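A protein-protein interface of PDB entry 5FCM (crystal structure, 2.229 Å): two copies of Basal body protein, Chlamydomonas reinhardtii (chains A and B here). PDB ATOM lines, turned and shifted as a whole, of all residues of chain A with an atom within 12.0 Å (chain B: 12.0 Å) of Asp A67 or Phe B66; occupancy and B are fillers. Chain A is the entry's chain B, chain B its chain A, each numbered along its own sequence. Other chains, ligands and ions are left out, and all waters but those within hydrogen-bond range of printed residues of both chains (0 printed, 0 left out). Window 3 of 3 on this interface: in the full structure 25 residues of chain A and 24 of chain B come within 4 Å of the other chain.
The side-chain amide nitrogen of Gln B55 lies close to the side-chain amide nitrogen of Gln B59, at 3.4 Å.
Cys A56 touches Gln B55. Gln A59 touches Ile B63. CG2 of Ile B63 touches OE2 of Glu A62 (3.7 Å). Gln B59 touches Ile A63 (CB to CD1, 3.9 Å). Glu B62 touches Ile A63. Ile B63 touches Ile A63. CD2 of Phe B66 touches CD2 of Phe A66 (3.3 Å). CZ of Phe B66 touches OD1 of Asp A67, 3.6 Å away.
NE2 of Gln A59 lies within hydrogen-bond range of O of Cys B56 (3.3 Å). OE1 of Gln B59 sits close to O of Cys A56 (3.2 Å). SG of Cys A56 sits close to N of Cys B56. NE2 of Gln A59 sits at hydrogen-bond distance from OE1 of Gln B59 (2.7 Å).
Gln A59 touches its own counterpart, Gln B59. Gln A59 touches Ile B63, and with the chains exchanged Ile A63 touches Gln B59. Ile B63 touches its own counterpart, Ile A63. Asp A67 touches Phe B66, but with the chains exchanged Phe A66 does not touch Asp B67 (4.4 Å). Of the 12 pairs that touch across the chains among the printed residues, 10 have their exchanged pair printed and touching as well.
Asp A67 touches just one residue of chain B: Phe B66. Phe B66 touches two residues of chain A. Of chain B, only Gln B59 (3.9 Å), Glu B62 (3.4 Å) and Ile B63 (3.6 Å) come within 4 Å of Ile A63. No residue of chain A comes within 4 Å of Ala B64. No residue of chain A comes within 4 Å of Ala B65. No residue of chain A comes within 4 Å of Asp B67. No residue of chain A comes within 4 Å of Leu B70. Printed residues of chain A within 4 Å of Cys B56: Cys A56 and Gln A59. Printed residues of chain B within 4 Å of Glu A62: Ile B63 (3.7 Å). Printed residues of chain B within 4 Å of Cys A56: Gln B55, Cys B56 and Gln B59. Printed residues of chain A within 4 Å of Gln B59: Cys A56 (3.2 Å), Gln A59 (2.7 Å) and Ile A63 (3.9 Å). Of the printed residues of chain B, Gln A59 touches Cys B56, Gln B59 and Ile B63. The nearest residue of chain A that does not touch Phe B66 is Ile A63 (4.5 Å).
Hydrophobic or aromatic side chains of chain A within 4 Å of the printed part of chain B: Ile A63 and Phe A66.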
ATOM      1  N   CYS A  56     -18.608  38.549 -24.320  1.00  0.00           N
ATOM      2  CA  CYS A  56     -19.198  37.467 -25.099  1.00  0.00           C
ATOM      3  C   CYS A  56     -18.989  37.707 -26.589  1.00  0.00           C
ATOM      4  O   CYS A  56     -18.708  36.776 -27.343  1.00  0.00           O
ATOM      5  CB  CYS A  56     -20.692  37.328 -24.798  1.00  0.00           C
ATOM      6  SG  CYS A  56     -21.070  36.584 -23.196  1.00  0.00           S
ATOM      7  N   LYS A  58     -16.542  39.392 -28.032  1.00  0.00           N
ATOM      8  CA  LYS A  58     -15.142  39.079 -28.291  1.00  0.00           C
ATOM      9  C   LYS A  58     -14.932  37.574 -28.422  1.00  0.00           C
ATOM     10  O   LYS A  58     -14.332  37.100 -29.388  1.00  0.00           O
ATOM     11  CB  LYS A  58     -14.255  39.633 -27.175  1.00  0.00           C
ATOM     12  CG  LYS A  58     -13.781  41.061 -27.398  1.00  0.00           C
ATOM     13  CD  LYS A  58     -14.041  41.939 -26.182  1.00  0.00           C
ATOM     14  CE  LYS A  58     -13.180  43.193 -26.206  1.00  0.00           C
ATOM     15  NZ  LYS A  58     -13.554  44.148 -25.127  1.00  0.00           N
ATOM     16  N   GLN A  59     -15.428  36.829 -27.440  1.00  0.00           N
ATOM     17  CA  GLN A  59     -15.294  35.379 -27.433  1.00  0.00           C
ATOM     18  C   GLN A  59     -15.987  34.759 -28.637  1.00  0.00           C
ATOM     19  O   GLN A  59     -15.529  33.752 -29.177  1.00  0.00           O
ATOM     20  CB  GLN A  59     -15.870  34.799 -26.142  1.00  0.00           C
ATOM     21  CG  GLN A  59     -15.064  35.153 -24.898  1.00  0.00           C
ATOM     22  CD  GLN A  59     -15.677  34.634 -23.604  1.00  0.00           C
ATOM     23  OE1 GLN A  59     -14.966  34.424 -22.622  1.00  0.00           O
ATOM     24  NE2 GLN A  59     -16.994  34.437 -23.591  1.00  0.00           N
ATOM     25  N   ALA A  60     -17.095  35.359 -29.055  1.00  0.00           N
ATOM     26  CA  ALA A  60     -17.835  34.858 -30.205  1.00  0.00           C
ATOM     27  C   ALA A  60     -16.984  34.973 -31.470  1.00  0.00           C
ATOM     28  O   ALA A  60     -16.984  34.073 -32.311  1.00  0.00           O
ATOM     29  CB  ALA A  60     -19.140  35.611 -30.367  1.00  0.00           C
ATOM     30  N   GLN A  61     -16.256  36.079 -31.594  1.00  0.00           N
ATOM     31  CA  GLN A  61     -15.348  36.276 -32.719  1.00  0.00           C
ATOM     32  C   GLN A  61     -14.204  35.274 -32.663  1.00  0.00           C
ATOM     33  O   GLN A  61     -13.836  34.674 -33.672  1.00  0.00           O
ATOM     34  CB  GLN A  61     -14.786  37.698 -32.725  1.00  0.00           C
ATOM     35  CG  GLN A  61     -15.815  38.779 -33.000  1.00  0.00           C
ATOM     36  CD  GLN A  61     -15.176  40.118 -33.313  1.00  0.00           C
ATOM     37  OE1 GLN A  61     -13.970  40.203 -33.545  1.00  0.00           O
ATOM     38  NE2 GLN A  61     -15.983  41.172 -33.321  1.00  0.00           N
ATOM     39  N   GLU A  62     -13.641  35.112 -31.470  1.00  0.00           N
ATOM     40  CA  GLU A  62     -12.522  34.202 -31.259  1.00  0.00           C
ATOM     41  C   GLU A  62     -12.926  32.774 -31.614  1.00  0.00           C
ATOM     42  O   GLU A  62     -12.128  32.007 -32.154  1.00  0.00           O
ATOM     43  CB  GLU A  62     -12.042  34.283 -29.806  1.00  0.00           C
ATOM     44  CG  GLU A  62     -10.770  33.501 -29.518  1.00  0.00           C
ATOM     45  CD  GLU A  62     -10.279  33.682 -28.092  1.00  0.00           C
ATOM     46  OE1 GLU A  62     -10.882  34.488 -27.349  1.00  0.00           O
ATOM     47  OE2 GLU A  62      -9.249  33.058 -27.760  1.00  0.00           O
ATOM     48  N   ILE A  63     -14.173  32.431 -31.311  1.00  0.00           N
ATOM     49  CA  ILE A  63     -14.698  31.103 -31.597  1.00  0.00           C
ATOM     50  C   ILE A  63     -14.941  30.960 -33.095  1.00  0.00           C
ATOM     51  O   ILE A  63     -14.732  29.890 -33.664  1.00  0.00           O
ATOM     52  CB  ILE A  63     -15.983  30.838 -30.786  1.00  0.00           C
ATOM     53  CG1 ILE A  63     -15.634  30.652 -29.309  1.00  0.00           C
ATOM     54  CG2 ILE A  63     -16.719  29.600 -31.302  1.00  0.00           C
ATOM     55  CD1 ILE A  63     -16.829  30.689 -28.380  1.00  0.00           C
ATOM     56  N   ALA A  64     -15.381  32.044 -33.728  1.00  0.00           N
ATOM     57  CA  ALA A  64     -15.634  32.043 -35.164  1.00  0.00           C
ATOM     58  C   ALA A  64     -14.331  31.879 -35.942  1.00  0.00           C
ATOM     59  O   ALA A  64     -14.321  31.337 -37.046  1.00  0.00           O
ATOM     60  CB  ALA A  64     -16.341  33.325 -35.578  1.00  0.00           C
ATOM     61  N   ALA A  65     -13.235  32.350 -35.356  1.00  0.00           N
ATOM     62  CA  ALA A  65     -11.928  32.266 -35.993  1.00  0.00           C
ATOM     63  C   ALA A  65     -11.360  30.855 -35.884  1.00  0.00           C
ATOM     64  O   ALA A  65     -10.731  30.360 -36.819  1.00  0.00           O
ATOM     65  CB  ALA A  65     -10.971  33.271 -35.370  1.00  0.00           C
ATOM     66  N   PHE A  66     -11.576  30.214 -34.740  1.00  0.00           N
ATOM     67  CA  PHE A  66     -11.117  28.844 -34.537  1.00  0.00           C
ATOM     68  C   PHE A  66     -11.758  27.908 -35.557  1.00  0.00           C
ATOM     69  O   PHE A  66     -11.086  27.055 -36.138  1.00  0.00           O
ATOM     70  CB  PHE A  66     -11.441  28.366 -33.119  1.00  0.00           C
ATOM     71  CG  PHE A  66     -10.416  28.762 -32.087  1.00  0.00           C
ATOM     72  CD1 PHE A  66      -9.064  28.556 -32.310  1.00  0.00           C
ATOM     73  CD2 PHE A  66     -10.811  29.332 -30.888  1.00  0.00           C
ATOM     74  CE1 PHE A  66      -8.125  28.916 -31.359  1.00  0.00           C
ATOM     75  CE2 PHE A  66      -9.878  29.694 -29.934  1.00  0.00           C
ATOM     76  CZ  PHE A  66      -8.534  29.487 -30.169  1.00  0.00           C
ATOM     77  N   ASP A  67     -13.059  28.074 -35.769  1.00  0.00           N
ATOM     78  CA  ASP A  67     -13.794  27.245 -36.717  1.00  0.00           C
ATOM     79  C   ASP A  67     -13.179  27.321 -38.111  1.00  0.00           C
ATOM     80  O   ASP A  67     -12.696  26.320 -38.641  1.00  0.00           O
ATOM     81  CB  ASP A  67     -15.263  27.672 -36.767  1.00  0.00           C
ATOM     82  CG  ASP A  67     -16.015  27.320 -35.498  1.00  0.00           C
ATOM     83  OD1 ASP A  67     -15.360  27.110 -34.455  1.00  0.00           O
ATOM     84  OD2 ASP A  67     -17.261  27.256 -35.543  1.00  0.00           O
ATOM     85  N   THR A  68     -13.199  28.513 -38.698  1.00  0.00           N
ATOM     86  CA  THR A  68     -12.669  28.713 -40.043  1.00  0.00           C
ATOM     87  C   THR A  68     -11.144  28.698 -40.032  1.00  0.00           C
ATOM     88  O   THR A  68     -10.526  27.828 -39.419  1.00  0.00           O
ATOM     89  CB  THR A  68     -13.155  30.045 -40.650  1.00  0.00           C
ATOM     90  OG1 THR A  68     -12.594  31.143 -39.921  1.00  0.00           O
ATOM     91  CG2 THR A  68     -14.676  30.134 -40.612  1.00  0.00           C
ATOM     92  N   GLN B  55     -23.564  32.369 -20.455  1.00  0.00           N
ATOM     93  CA  GLN B  55     -23.172  32.397 -21.857  1.00  0.00           C
ATOM     94  C   GLN B  55     -21.660  32.532 -21.964  1.00  0.00           C
ATOM     95  O   GLN B  55     -20.997  31.758 -22.654  1.00  0.00           O
ATOM     96  CB  GLN B  55     -23.870  33.559 -22.573  1.00  0.00           C
ATOM     97  CG  GLN B  55     -23.419  33.820 -24.007  1.00  0.00           C
ATOM     98  CD  GLN B  55     -23.883  32.752 -24.977  1.00  0.00           C
ATOM     99  OE1 GLN B  55     -24.228  31.639 -24.579  1.00  0.00           O
ATOM    100  NE2 GLN B  55     -23.901  33.093 -26.261  1.00  0.00           N
ATOM    101  N   CYS B  56     -21.128  33.529 -21.269  1.00  0.00           N
ATOM    102  CA  CYS B  56     -19.699  33.796 -21.265  1.00  0.00           C
ATOM    103  C   CYS B  56     -18.922  32.588 -20.755  1.00  0.00           C
ATOM    104  O   CYS B  56     -17.844  32.273 -21.258  1.00  0.00           O
ATOM    105  CB  CYS B  56     -19.400  35.023 -20.403  1.00  0.00           C
ATOM    106  SG  CYS B  56     -17.679  35.549 -20.412  1.00  0.00           S
ATOM    107  N   ALA B  57     -19.482  31.912 -19.757  1.00  0.00           N
ATOM    108  CA  ALA B  57     -18.831  30.755 -19.154  1.00  0.00           C
ATOM    109  C   ALA B  57     -18.789  29.584 -20.130  1.00  0.00           C
ATOM    110  O   ALA B  57     -17.785  28.882 -20.221  1.00  0.00           O
ATOM    111  CB  ALA B  57     -19.549  30.353 -17.872  1.00  0.00           C
ATOM    112  N   LYS B  58     -19.883  29.378 -20.855  1.00  0.00           N
ATOM    113  CA  LYS B  58     -19.949  28.308 -21.841  1.00  0.00           C
ATOM    114  C   LYS B  58     -18.978  28.572 -22.989  1.00  0.00           C
ATOM    115  O   LYS B  58     -18.330  27.652 -23.490  1.00  0.00           O
ATOM    116  CB  LYS B  58     -21.372  28.157 -22.383  1.00  0.00           C
ATOM    117  CG  LYS B  58     -22.381  27.663 -21.360  1.00  0.00           C
ATOM    118  CD  LYS B  58     -23.743  27.412 -21.997  1.00  0.00           C
ATOM    119  CE  LYS B  58     -24.805  27.093 -20.953  1.00  0.00           C
ATOM    120  NZ  LYS B  58     -24.440  25.929 -20.097  1.00  0.00           N
ATOM    121  N   GLN B  59     -18.878  29.831 -23.403  1.00  0.00           N
ATOM    122  CA  GLN B  59     -17.962  30.206 -24.474  1.00  0.00           C
ATOM    123  C   GLN B  59     -16.512  30.000 -24.054  1.00  0.00           C
ATOM    124  O   GLN B  59     -15.688  29.551 -24.850  1.00  0.00           O
ATOM    125  CB  GLN B  59     -18.184  31.658 -24.885  1.00  0.00           C
ATOM    126  CG  GLN B  59     -19.467  31.894 -25.651  1.00  0.00           C
ATOM    127  CD  GLN B  59     -19.678  33.357 -25.964  1.00  0.00           C
ATOM    128  OE1 GLN B  59     -19.015  34.226 -25.397  1.00  0.00           O
ATOM    129  NE2 GLN B  59     -20.602  33.641 -26.871  1.00  0.00           N
ATOM    130  N   ALA B  60     -16.202  30.337 -22.807  1.00  0.00           N
ATOM    131  CA  ALA B  60     -14.860  30.126 -22.279  1.00  0.00           C
ATOM    132  C   ALA B  60     -14.510  28.642 -22.313  1.00  0.00           C
ATOM    133  O   ALA B  60     -13.361  28.269 -22.553  1.00  0.00           O
ATOM    134  CB  ALA B  60     -14.751  30.663 -20.864  1.00  0.00           C
ATOM    135  N   GLN B  61     -15.510  27.802 -22.070  1.00  0.00           N
ATOM    136  CA  GLN B  61     -15.328  26.355 -22.097  1.00  0.00           C
ATOM    137  C   GLN B  61     -15.053  25.883 -23.521  1.00  0.00           C
ATOM    138  O   GLN B  61     -14.203  25.024 -23.747  1.00  0.00           O
ATOM    139  CB  GLN B  61     -16.564  25.649 -21.532  1.00  0.00           C
ATOM    140  CG  GLN B  61     -16.767  25.857 -20.037  1.00  0.00           C
ATOM    141  CD  GLN B  61     -18.155  25.455 -19.569  1.00  0.00           C
ATOM    142  OE1 GLN B  61     -18.966  24.947 -20.345  1.00  0.00           O
ATOM    143  NE2 GLN B  61     -18.435  25.686 -18.291  1.00  0.00           N
ATOM    144  N   GLU B  62     -15.779  26.456 -24.477  1.00  0.00           N
ATOM    145  CA  GLU B  62     -15.604  26.114 -25.884  1.00  0.00           C
ATOM    146  C   GLU B  62     -14.221  26.536 -26.374  1.00  0.00           C
ATOM    147  O   GLU B  62     -13.587  25.828 -27.155  1.00  0.00           O
ATOM    148  CB  GLU B  62     -16.694  26.776 -26.733  1.00  0.00           C
ATOM    149  CG  GLU B  62     -18.099  26.261 -26.439  1.00  0.00           C
ATOM    150  CD  GLU B  62     -19.193  27.119 -27.049  1.00  0.00           C
ATOM    151  OE1 GLU B  62     -18.867  28.062 -27.801  1.00  0.00           O
ATOM    152  OE2 GLU B  62     -20.380  26.849 -26.771  1.00  0.00           O
ATOM    153  N   ILE B  63     -13.757  27.689 -25.902  1.00  0.00           N
ATOM    154  CA  ILE B  63     -12.457  28.216 -26.298  1.00  0.00           C
ATOM    155  C   ILE B  63     -11.352  27.326 -25.747  1.00  0.00           C
ATOM    156  O   ILE B  63     -10.427  26.949 -26.468  1.00  0.00           O
ATOM    157  CB  ILE B  63     -12.286  29.675 -25.828  1.00  0.00           C
ATOM    158  CG1 ILE B  63     -13.242  30.587 -26.599  1.00  0.00           C
ATOM    159  CG2 ILE B  63     -10.848  30.153 -26.032  1.00  0.00           C
ATOM    160  CD1 ILE B  63     -13.413  31.962 -25.984  1.00  0.00           C
ATOM    161  N   ALA B  64     -11.447  26.993 -24.465  1.00  0.00           N
ATOM    162  CA  ALA B  64     -10.447  26.147 -23.826  1.00  0.00           C
ATOM    163  C   ALA B  64     -10.425  24.755 -24.456  1.00  0.00           C
ATOM    164  O   ALA B  64      -9.422  24.047 -24.375  1.00  0.00           O
ATOM    165  CB  ALA B  64     -10.715  26.051 -22.334  1.00  0.00           C
ATOM    166  N   ALA B  65     -11.533  24.369 -25.082  1.00  0.00           N
ATOM    167  CA  ALA B  65     -11.636  23.066 -25.733  1.00  0.00           C
ATOM    168  C   ALA B  65     -10.777  23.002 -26.995  1.00  0.00           C
ATOM    169  O   ALA B  65     -10.338  21.926 -27.396  1.00  0.00           O
ATOM    170  CB  ALA B  65     -13.082  22.760 -26.070  1.00  0.00           C
ATOM    171  N   PHE B  66     -10.552  24.152 -27.622  1.00  0.00           N
ATOM    172  CA  PHE B  66      -9.690  24.226 -28.796  1.00  0.00           C
ATOM    173  C   PHE B  66      -8.225  24.078 -28.412  1.00  0.00           C
ATOM    174  O   PHE B  66      -7.455  23.409 -29.101  1.00  0.00           O
ATOM    175  CB  PHE B  66      -9.888  25.552 -29.531  1.00  0.00           C
ATOM    176  CG  PHE B  66     -11.220  25.681 -30.207  1.00  0.00           C
ATOM    177  CD1 PHE B  66     -11.509  24.946 -31.344  1.00  0.00           C
ATOM    178  CD2 PHE B  66     -12.174  26.557 -29.718  1.00  0.00           C
ATOM    179  CE1 PHE B  66     -12.731  25.072 -31.974  1.00  0.00           C
ATOM    180  CE2 PHE B  66     -13.396  26.690 -30.344  1.00  0.00           C
ATOM    181  CZ  PHE B  66     -13.676  25.948 -31.474  1.00  0.00           C
ATOM    182  N   ASP B  67      -7.846  24.721 -27.313  1.00  0.00           N
ATOM    183  CA  ASP B  67      -6.464  24.712 -26.848  1.00  0.00           C
ATOM    184  C   ASP B  67      -5.942  23.291 -26.661  1.00  0.00           C
ATOM    185  O   ASP B  67      -4.769  23.013 -26.908  1.00  0.00           O
ATOM    186  CB  ASP B  67      -6.343  25.487 -25.533  1.00  0.00           C
ATOM    187  CG  ASP B  67      -6.899  26.895 -25.631  1.00  0.00           C
ATOM    188  OD1 ASP B  67      -7.655  27.173 -26.587  1.00  0.00           O
ATOM    189  OD2 ASP B  67      -6.587  27.723 -24.748  1.00  0.00           O
ATOM    190  N   THR B  68      -6.820  22.395 -26.222  1.00  0.00           N
ATOM    191  CA  THR B  68      -6.431  21.015 -25.951  1.00  0.00           C
ATOM    192  C   THR B  68      -6.308  20.221 -27.246  1.00  0.00           C
ATOM    193  O   THR B  68      -5.459  19.336 -27.361  1.00  0.00           O
ATOM    194  CB  THR B  68      -7.442  20.318 -25.028  1.00  0.00           C
ATOM    195  OG1 THR B  68      -8.660  20.080 -25.742  1.00  0.00           O
ATOM    196  CG2 THR B  68      -7.731  21.180 -23.812  1.00  0.00           C
ATOM    197  N   ARG B  69      -7.157  20.541 -28.218  1.00  0.00           N
ATOM    198  CA  ARG B  69      -7.088  19.904 -29.529  1.00  0.00           C
ATOM    199  C   ARG B  69      -5.742  20.198 -30.191  1.00  0.00           C
ATOM    200  O   ARG B  69      -5.345  19.520 -31.139  1.00  0.00           O
ATOM    201  CB  ARG B  69      -8.240  20.378 -30.422  1.00  0.00           C
ATOM    202  CG  ARG B  69      -9.616  20.137 -29.821  1.00  0.00           C
ATOM    203  CD  ARG B  69     -10.553  19.430 -30.789  1.00  0.00           C
ATOM    204  NE  ARG B  69     -11.011  20.307 -31.865  1.00  0.00           N
ATOM    205  CZ  ARG B  69     -11.804  19.920 -32.860  1.00  0.00           C
ATOM    206  NH1 ARG B  69     -12.230  18.665 -32.927  1.00  0.00           N
ATOM    207  NH2 ARG B  69     -12.171  20.788 -33.792  1.00  0.00           N
ATOM    208  N   LEU B  70      -5.050  21.217 -29.687  1.00  0.00           N
ATOM    209  CA  LEU B  70      -3.695  21.528 -30.128  1.00  0.00           C
ATOM    210  C   LEU B  70      -2.770  21.698 -28.926  1.00  0.00           C
ATOM    211  O   LEU B  70      -2.563  20.763 -28.152  1.00  0.00           O
ATOM    212  CB  LEU B  70      -3.683  22.793 -30.984  1.00  0.00           C
ATOM    213  CG  LEU B  70      -4.374  22.672 -32.342  1.00  0.00           C
ATOM    214  CD1 LEU B  70      -5.635  23.521 -32.385  1.00  0.00           C
ATOM    215  CD2 LEU B  70      -3.417  23.064 -33.457  1.00  0.00           C
